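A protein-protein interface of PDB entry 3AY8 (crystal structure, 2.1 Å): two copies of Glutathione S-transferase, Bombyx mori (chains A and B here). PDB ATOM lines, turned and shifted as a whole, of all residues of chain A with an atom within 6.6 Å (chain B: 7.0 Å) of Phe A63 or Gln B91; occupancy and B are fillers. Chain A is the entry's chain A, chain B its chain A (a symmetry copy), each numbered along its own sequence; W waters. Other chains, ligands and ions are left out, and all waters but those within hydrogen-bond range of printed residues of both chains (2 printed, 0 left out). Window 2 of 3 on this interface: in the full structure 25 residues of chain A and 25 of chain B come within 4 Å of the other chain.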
ATOM      1  N   LEU A  58      -1.241  15.211 -16.531  1.00  0.00           N
ATOM      2  CA  LEU A  58      -0.315  14.554 -17.417  1.00  0.00           C
ATOM      3  C   LEU A  58      -0.323  13.044 -17.131  1.00  0.00           C
ATOM      4  O   LEU A  58      -0.262  12.627 -15.974  1.00  0.00           O
ATOM      5  CB  LEU A  58       1.088  15.123 -17.209  1.00  0.00           C
ATOM      6  CG  LEU A  58       2.209  14.669 -18.149  1.00  0.00           C
ATOM      7  CD1 LEU A  58       2.108  15.344 -19.524  1.00  0.00           C
ATOM      8  CD2 LEU A  58       3.563  14.930 -17.520  1.00  0.00           C
ATOM      9  N   ASP A  59      -0.421  12.241 -18.186  1.00  0.00           N
ATOM     10  CA  ASP A  59      -0.174  10.795 -18.091  1.00  0.00           C
ATOM     11  C   ASP A  59       1.082  10.465 -18.897  1.00  0.00           C
ATOM     12  O   ASP A  59       1.047  10.390 -20.129  1.00  0.00           O
ATOM     13  CB  ASP A  59      -1.378   9.996 -18.600  1.00  0.00           C
ATOM     14  CG  ASP A  59      -1.228   8.480 -18.386  1.00  0.00           C
ATOM     15  OD1 ASP A  59      -0.097   7.971 -18.209  1.00  0.00           O
ATOM     16  OD2 ASP A  59      -2.260   7.792 -18.397  1.00  0.00           O
ATOM     17  N   ASP A  60       2.197  10.317 -18.189  1.00  0.00           N
ATOM     18  CA  ASP A  60       3.456   9.928 -18.797  1.00  0.00           C
ATOM     19  C   ASP A  60       3.697   8.445 -18.526  1.00  0.00           C
ATOM     20  O   ASP A  60       4.313   8.083 -17.511  1.00  0.00           O
ATOM     21  CB  ASP A  60       4.609  10.753 -18.223  1.00  0.00           C
ATOM     22  CG  ASP A  60       5.958  10.364 -18.809  1.00  0.00           C
ATOM     23  OD1 ASP A  60       6.015   9.477 -19.687  1.00  0.00           O
ATOM     24  OD2 ASP A  60       6.973  10.942 -18.390  1.00  0.00           O
ATOM     25  N   ASN A  61       3.184   7.598 -19.421  1.00  0.00           N
ATOM     26  CA  ASN A  61       3.411   6.146 -19.360  1.00  0.00           C
ATOM     27  C   ASN A  61       2.930   5.592 -18.011  1.00  0.00           C
ATOM     28  O   ASN A  61       3.644   4.851 -17.332  1.00  0.00           O
ATOM     29  CB  ASN A  61       4.893   5.811 -19.618  1.00  0.00           C
ATOM     30  CG  ASN A  61       5.405   6.308 -20.996  1.00  0.00           C
ATOM     31  OD1 ASN A  61       5.949   5.528 -21.778  1.00  0.00           O
ATOM     32  ND2 ASN A  61       5.245   7.606 -21.282  1.00  0.00           N
ATOM     33  N   ASN A  62       1.719   5.999 -17.628  1.00  0.00           N
ATOM     34  CA  ASN A  62       1.084   5.642 -16.347  1.00  0.00           C
ATOM     35  C   ASN A  62       1.527   6.369 -15.061  1.00  0.00           C
ATOM     36  O   ASN A  62       0.884   6.208 -14.020  1.00  0.00           O
ATOM     37  CB  ASN A  62       0.997   4.122 -16.154  1.00  0.00           C
ATOM     38  CG  ASN A  62      -0.015   3.495 -17.088  1.00  0.00           C
ATOM     39  OD1 ASN A  62      -1.163   3.263 -16.703  1.00  0.00           O
ATOM     40  ND2 ASN A  62       0.380   3.281 -18.343  1.00  0.00           N
ATOM     41  N   PHE A  63       2.593   7.162 -15.134  1.00  0.00           N
ATOM     42  CA  PHE A  63       2.865   8.170 -14.096  1.00  0.00           C
ATOM     43  C   PHE A  63       1.907   9.329 -14.340  1.00  0.00           C
ATOM     44  O   PHE A  63       2.010  10.041 -15.346  1.00  0.00           O
ATOM     45  CB  PHE A  63       4.325   8.655 -14.116  1.00  0.00           C
ATOM     46  CG  PHE A  63       4.605   9.812 -13.168  1.00  0.00           C
ATOM     47  CD1 PHE A  63       4.485   9.652 -11.786  1.00  0.00           C
ATOM     48  CD2 PHE A  63       5.006  11.050 -13.663  1.00  0.00           C
ATOM     49  CE1 PHE A  63       4.740  10.717 -10.906  1.00  0.00           C
ATOM     50  CE2 PHE A  63       5.268  12.126 -12.798  1.00  0.00           C
ATOM     51  CZ  PHE A  63       5.129  11.952 -11.414  1.00  0.00           C
ATOM     52  N   VAL A  64       0.962   9.481 -13.425  1.00  0.00           N
ATOM     53  CA  VAL A  64      -0.090  10.479 -13.526  1.00  0.00           C
ATOM     54  C   VAL A  64       0.253  11.657 -12.622  1.00  0.00           C
ATOM     55  O   VAL A  64       0.515  11.489 -11.426  1.00  0.00           O
ATOM     56  CB  VAL A  64      -1.451   9.885 -13.123  1.00  0.00           C
ATOM     57  CG1 VAL A  64      -2.541  10.952 -13.143  1.00  0.00           C
ATOM     58  CG2 VAL A  64      -1.815   8.722 -14.047  1.00  0.00           C
ATOM     59  N   LEU A  65       0.275  12.847 -13.215  1.00  0.00           N
ATOM     60  CA  LEU A  65       0.685  14.044 -12.508  1.00  0.00           C
ATOM     61  C   LEU A  65      -0.292  15.172 -12.793  1.00  0.00           C
ATOM     62  O   LEU A  65      -0.615  15.439 -13.946  1.00  0.00           O
ATOM     63  CB  LEU A  65       2.089  14.455 -12.964  1.00  0.00           C
ATOM     64  CG  LEU A  65       2.782  15.636 -12.285  1.00  0.00           C
ATOM     65  CD1 LEU A  65       3.139  15.304 -10.810  1.00  0.00           C
ATOM     66  CD2 LEU A  65       4.009  16.050 -13.089  1.00  0.00           C
ATOM     67  N   TYR A  74       8.503  19.064 -14.499  1.00  0.00           N
ATOM     68  CA  TYR A  74       8.737  17.652 -14.786  1.00  0.00           C
ATOM     69  C   TYR A  74       9.073  17.441 -16.272  1.00  0.00           C
ATOM     70  O   TYR A  74      10.060  16.773 -16.606  1.00  0.00           O
ATOM     71  CB  TYR A  74       7.516  16.826 -14.398  1.00  0.00           C
ATOM     72  CG  TYR A  74       7.610  15.391 -14.859  1.00  0.00           C
ATOM     73  CD1 TYR A  74       8.442  14.483 -14.198  1.00  0.00           C
ATOM     74  CD2 TYR A  74       6.893  14.947 -15.965  1.00  0.00           C
ATOM     75  CE1 TYR A  74       8.551  13.175 -14.630  1.00  0.00           C
ATOM     76  CE2 TYR A  74       6.993  13.635 -16.406  1.00  0.00           C
ATOM     77  CZ  TYR A  74       7.825  12.754 -15.732  1.00  0.00           C
ATOM     78  OH  TYR A  74       7.930  11.443 -16.140  1.00  0.00           O
ATOM     79  N   LYS A  78      12.623  16.187 -17.645  1.00  0.00           N
ATOM     80  CA  LYS A  78      12.571  14.862 -18.259  1.00  0.00           C
ATOM     81  C   LYS A  78      12.858  14.883 -19.777  1.00  0.00           C
ATOM     82  O   LYS A  78      13.586  14.023 -20.277  1.00  0.00           O
ATOM     83  CB  LYS A  78      11.240  14.160 -17.940  1.00  0.00           C
ATOM     84  CG  LYS A  78      11.124  12.727 -18.464  1.00  0.00           C
ATOM     85  CD  LYS A  78      11.530  11.694 -17.437  1.00  0.00           C
ATOM     86  CE  LYS A  78      11.493  10.287 -18.024  1.00  0.00           C
ATOM     87  NZ  LYS A  78      10.087   9.789 -18.256  1.00  0.00           N
ATOM     88  N   PRO B  87      13.470  14.542  -2.996  1.00  0.00           N
ATOM     89  CA  PRO B  87      14.140  13.515  -3.823  1.00  0.00           C
ATOM     90  C   PRO B  87      14.531  13.996  -5.214  1.00  0.00           C
ATOM     91  O   PRO B  87      13.785  14.759  -5.847  1.00  0.00           O
ATOM     92  CB  PRO B  87      13.113  12.385  -3.901  1.00  0.00           C
ATOM     93  CG  PRO B  87      12.292  12.540  -2.647  1.00  0.00           C
ATOM     94  CD  PRO B  87      12.193  14.053  -2.447  1.00  0.00           C
ATOM     95  N   LYS B  88      15.699  13.548  -5.670  1.00  0.00           N
ATOM     96  CA  LYS B  88      16.215  13.957  -6.966  1.00  0.00           C
ATOM     97  C   LYS B  88      15.534  13.221  -8.116  1.00  0.00           C
ATOM     98  O   LYS B  88      15.455  13.767  -9.213  1.00  0.00           O
ATOM     99  CB  LYS B  88      17.735  13.811  -7.029  1.00  0.00           C
ATOM    100  CG  LYS B  88      18.448  14.623  -5.945  1.00  0.00           C
ATOM    101  CD  LYS B  88      19.916  14.873  -6.266  1.00  0.00           C
ATOM    102  CE  LYS B  88      20.182  16.354  -6.505  1.00  0.00           C
ATOM    103  NZ  LYS B  88      20.190  17.083  -5.209  1.00  0.00           N
ATOM    104  N   ASP B  89      15.036  12.007  -7.867  1.00  0.00           N
ATOM    105  CA  ASP B  89      14.231  11.274  -8.872  1.00  0.00           C
ATOM    106  C   ASP B  89      13.112  12.202  -9.382  1.00  0.00           C
ATOM    107  O   ASP B  89      12.395  12.807  -8.575  1.00  0.00           O
ATOM    108  CB  ASP B  89      13.646   9.979  -8.273  1.00  0.00           C
ATOM    109  CG  ASP B  89      12.660   9.266  -9.219  1.00  0.00           C
ATOM    110  OD1 ASP B  89      13.106   8.443 -10.052  1.00  0.00           O
ATOM    111  OD2 ASP B  89      11.434   9.504  -9.120  1.00  0.00           O
ATOM    112  N   LEU B  90      12.969  12.306 -10.704  1.00  0.00           N
ATOM    113  CA  LEU B  90      12.099  13.324 -11.298  1.00  0.00           C
ATOM    114  C   LEU B  90      10.629  13.128 -10.997  1.00  0.00           C
ATOM    115  O   LEU B  90       9.911  14.099 -10.826  1.00  0.00           O
ATOM    116  CB  LEU B  90      12.321  13.446 -12.817  1.00  0.00           C
ATOM    117  CG  LEU B  90      13.703  13.965 -13.208  1.00  0.00           C
ATOM    118  CD1 LEU B  90      13.847  14.032 -14.722  1.00  0.00           C
ATOM    119  CD2 LEU B  90      13.944  15.336 -12.573  1.00  0.00           C
ATOM    120  N   GLN B  91      10.187  11.878 -10.946  1.00  0.00           N
ATOM    121  CA  GLN B  91       8.804  11.566 -10.631  1.00  0.00           C
ATOM    122  C   GLN B  91       8.475  11.766  -9.134  1.00  0.00           C
ATOM    123  O   GLN B  91       7.432  12.341  -8.800  1.00  0.00           O
ATOM    124  CB  GLN B  91       8.432  10.165 -11.142  1.00  0.00           C
ATOM    125  CG  GLN B  91       8.623  10.019 -12.675  1.00  0.00           C
ATOM    126  CD  GLN B  91       8.063   8.722 -13.264  1.00  0.00           C
ATOM    127  OE1 GLN B  91       7.683   7.797 -12.538  1.00  0.00           O
ATOM    128  NE2 GLN B  91       8.006   8.659 -14.597  1.00  0.00           N
ATOM    129  N   LYS B  92       9.367  11.319  -8.249  1.00  0.00           N
ATOM    130  CA  LYS B  92       9.237  11.612  -6.817  1.00  0.00           C
ATOM    131  C   LYS B  92       9.322  13.122  -6.540  1.00  0.00           C
ATOM    132  O   LYS B  92       8.560  13.640  -5.736  1.00  0.00           O
ATOM    133  CB  LYS B  92      10.294  10.867  -5.997  1.00  0.00           C
ATOM    134  CG  LYS B  92      10.105   9.347  -5.974  1.00  0.00           C
ATOM    135  CD  LYS B  92      11.281   8.638  -5.295  1.00  0.00           C
ATOM    136  CE  LYS B  92      11.022   7.126  -5.230  1.00  0.00           C
ATOM    137  NZ  LYS B  92      12.186   6.383  -4.651  1.00  0.00           N
ATOM    138  N   ARG B  93      10.243  13.813  -7.207  1.00  0.00           N
ATOM    139  CA  ARG B  93      10.339  15.274  -7.102  1.00  0.00           C
ATOM    140  C   ARG B  93       9.043  15.960  -7.598  1.00  0.00           C
ATOM    141  O   ARG B  93       8.556  16.899  -6.974  1.00  0.00           O
ATOM    142  CB  ARG B  93      11.563  15.789  -7.853  1.00  0.00           C
ATOM    143  CG  ARG B  93      11.745  17.300  -7.816  1.00  0.00           C
ATOM    144  CD  ARG B  93      13.178  17.704  -8.108  1.00  0.00           C
ATOM    145  NE  ARG B  93      14.079  17.245  -7.052  1.00  0.00           N
ATOM    146  CZ  ARG B  93      15.182  17.877  -6.659  1.00  0.00           C
ATOM    147  NH1 ARG B  93      15.532  19.018  -7.224  1.00  0.00           N
ATOM    148  NH2 ARG B  93      15.925  17.372  -5.677  1.00  0.00           N
ATOM    149  N   ALA B  94       8.487  15.471  -8.704  1.00  0.00           N
ATOM    150  CA  ALA B  94       7.244  16.024  -9.257  1.00  0.00           C
ATOM    151  C   ALA B  94       6.079  15.937  -8.274  1.00  0.00           C
ATOM    152  O   ALA B  94       5.273  16.862  -8.174  1.00  0.00           O
ATOM    153  CB  ALA B  94       6.892  15.335 -10.570  1.00  0.00           C
ATOM    154  N   VAL B  95       6.013  14.844  -7.523  1.00  0.00           N
ATOM    155  CA  VAL B  95       4.976  14.696  -6.520  1.00  0.00           C
ATOM    156  C   VAL B  95       5.155  15.688  -5.371  1.00  0.00           C
ATOM    157  O   VAL B  95       4.185  16.294  -4.925  1.00  0.00           O
ATOM    158  CB  VAL B  95       4.834  13.231  -6.028  1.00  0.00           C
ATOM    159  CG1 VAL B  95       3.732  13.119  -4.993  1.00  0.00           C
ATOM    160  CG2 VAL B  95       4.492  12.307  -7.226  1.00  0.00           C
ATOM    161  N   VAL B  96       6.382  15.867  -4.898  1.00  0.00           N
ATOM    162  CA  VAL B  96       6.641  16.880  -3.867  1.00  0.00           C
ATOM    163  C   VAL B  96       6.304  18.286  -4.405  1.00  0.00           C
ATOM    164  O   VAL B  96       5.667  19.070  -3.720  1.00  0.00           O
ATOM    165  CB  VAL B  96       8.101  16.825  -3.362  1.00  0.00           C
ATOM    166  CG1 VAL B  96       8.405  18.012  -2.449  1.00  0.00           C
ATOM    167  CG2 VAL B  96       8.372  15.498  -2.641  1.00  0.00           C
ATOM    168  N   GLN B  98       4.248  19.052  -6.714  1.00  0.00           N
ATOM    169  CA  GLN B  98       2.793  19.031  -6.829  1.00  0.00           C
ATOM    170  C   GLN B  98       2.137  19.399  -5.498  1.00  0.00           C
ATOM    171  O   GLN B  98       1.273  20.281  -5.461  1.00  0.00           O
ATOM    172  CB  GLN B  98       2.318  17.656  -7.316  1.00  0.00           C
ATOM    173  CG  GLN B  98       0.851  17.547  -7.672  1.00  0.00           C
ATOM    174  CD  GLN B  98       0.375  16.097  -7.675  1.00  0.00           C
ATOM    175  OE1 GLN B  98       0.247  15.460  -6.621  1.00  0.00           O
ATOM    176  NE2 GLN B  98       0.136  15.568  -8.853  1.00  0.00           N
HETATM  177  O   HOH W   1       6.804   7.161 -16.611  1.00  0.00           O
HETATM  178  O   HOH W   2      -0.791  13.071  -9.576  1.00  0.00           O
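Water W2 lies within hydrogen-bond range of the side-chain amide nitrogen of Gln B98 and the backbone carbonyl oxygen of Val A64. Water W1 lies within hydrogen-bond range of NE2 of Gln B91 (2.8 Å) and O of Asp A60 (2.8 Å).
No position is printed for both chains. Of the 7 pairs that touch across the chains among the printed residues, none has its exchanged pair printed and touching as well.
The backbone NH (N) of Leu A58 sits at hydrogen-bond distance from the backbone carbonyl oxygen (O) of Leu A65 (2.7 Å). The side-chain hydroxyl (OH) of Tyr A74 lies within hydrogen-bond range of the side-chain carboxylate (OD2) of Asp A60 (2.5 Å). The side-chain amino group (NZ) of Lys A78 is in salt-bridge range of the side-chain carboxylate (OD2) of Asp A60 (3.3 Å). The side-chain amino group (NZ) of Lys A78 sits at hydrogen-bond distance from the side-chain hydroxyl (OH) of Tyr A74, at 3.4 Å. The side-chain carboxylate of Asp B89 sits at hydrogen-bond distance from the backbone NH of Gln B91 (3.2 Å).
The side-chain amide nitrogen (NE2) of Gln B91 is in hydrogen-bond range of the side-chain hydroxyl (OH) of Tyr A74.
Among the printed residues, merely in contact across the chains: Phe A63 with Gln B91, Phe A63 with Ala B94, Leu A65 with Ala B94, Leu A65 with Gln B98, Tyr A74 with Leu B90 and Lys A78 with Leu B90.
Printed residues of chain B within 4 Å of Phe A63: Gln B91 (3.5 Å) and Ala B94 (3.9 Å). Gln B91 touches just these residues of chain A: Phe A63 and Tyr A74. Printed residues of chain B within 4 Å of Lys A78: Leu B90. Printed residues of chain A within 4 Å of Leu B90: Tyr A74 (3.7 Å) and Lys A78 (3.8 Å). Printed residues of chain B within 4 Å of Leu A65: Ala B94 (3.7 Å) and Gln B98 (3.6 Å). Of the printed residues of chain A, Ala B94 touches Phe A63 and Leu A65. Of the printed residues of chain A, Gln B98 touches Leu A65 (3.6 Å). Arg B93 touches none of the printed residues of chain A. Lys B88 touches none of the printed residues of chain A. The nearest residue of chain A that does not touch Gln B91 is Lys A78 (4.4 Å). The nearest printed residue of chain A that does not touch Gln B98 is Val A64 (4.8 Å).
Of the 10 printed residues of chain A, 4 touch a printed residue of chain B. Hydrophobic or aromatic side chains of chain A that line the printed part of chain B: Phe A63, Leu A65 and Tyr A74. Of the 11 printed residues of chain B, 4 touch a printed residue of chain A. Among the printed residues, no Asp or Glu carboxylate lies within 4 Å of a Lys or Arg side-chain nitrogen of the other chain.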
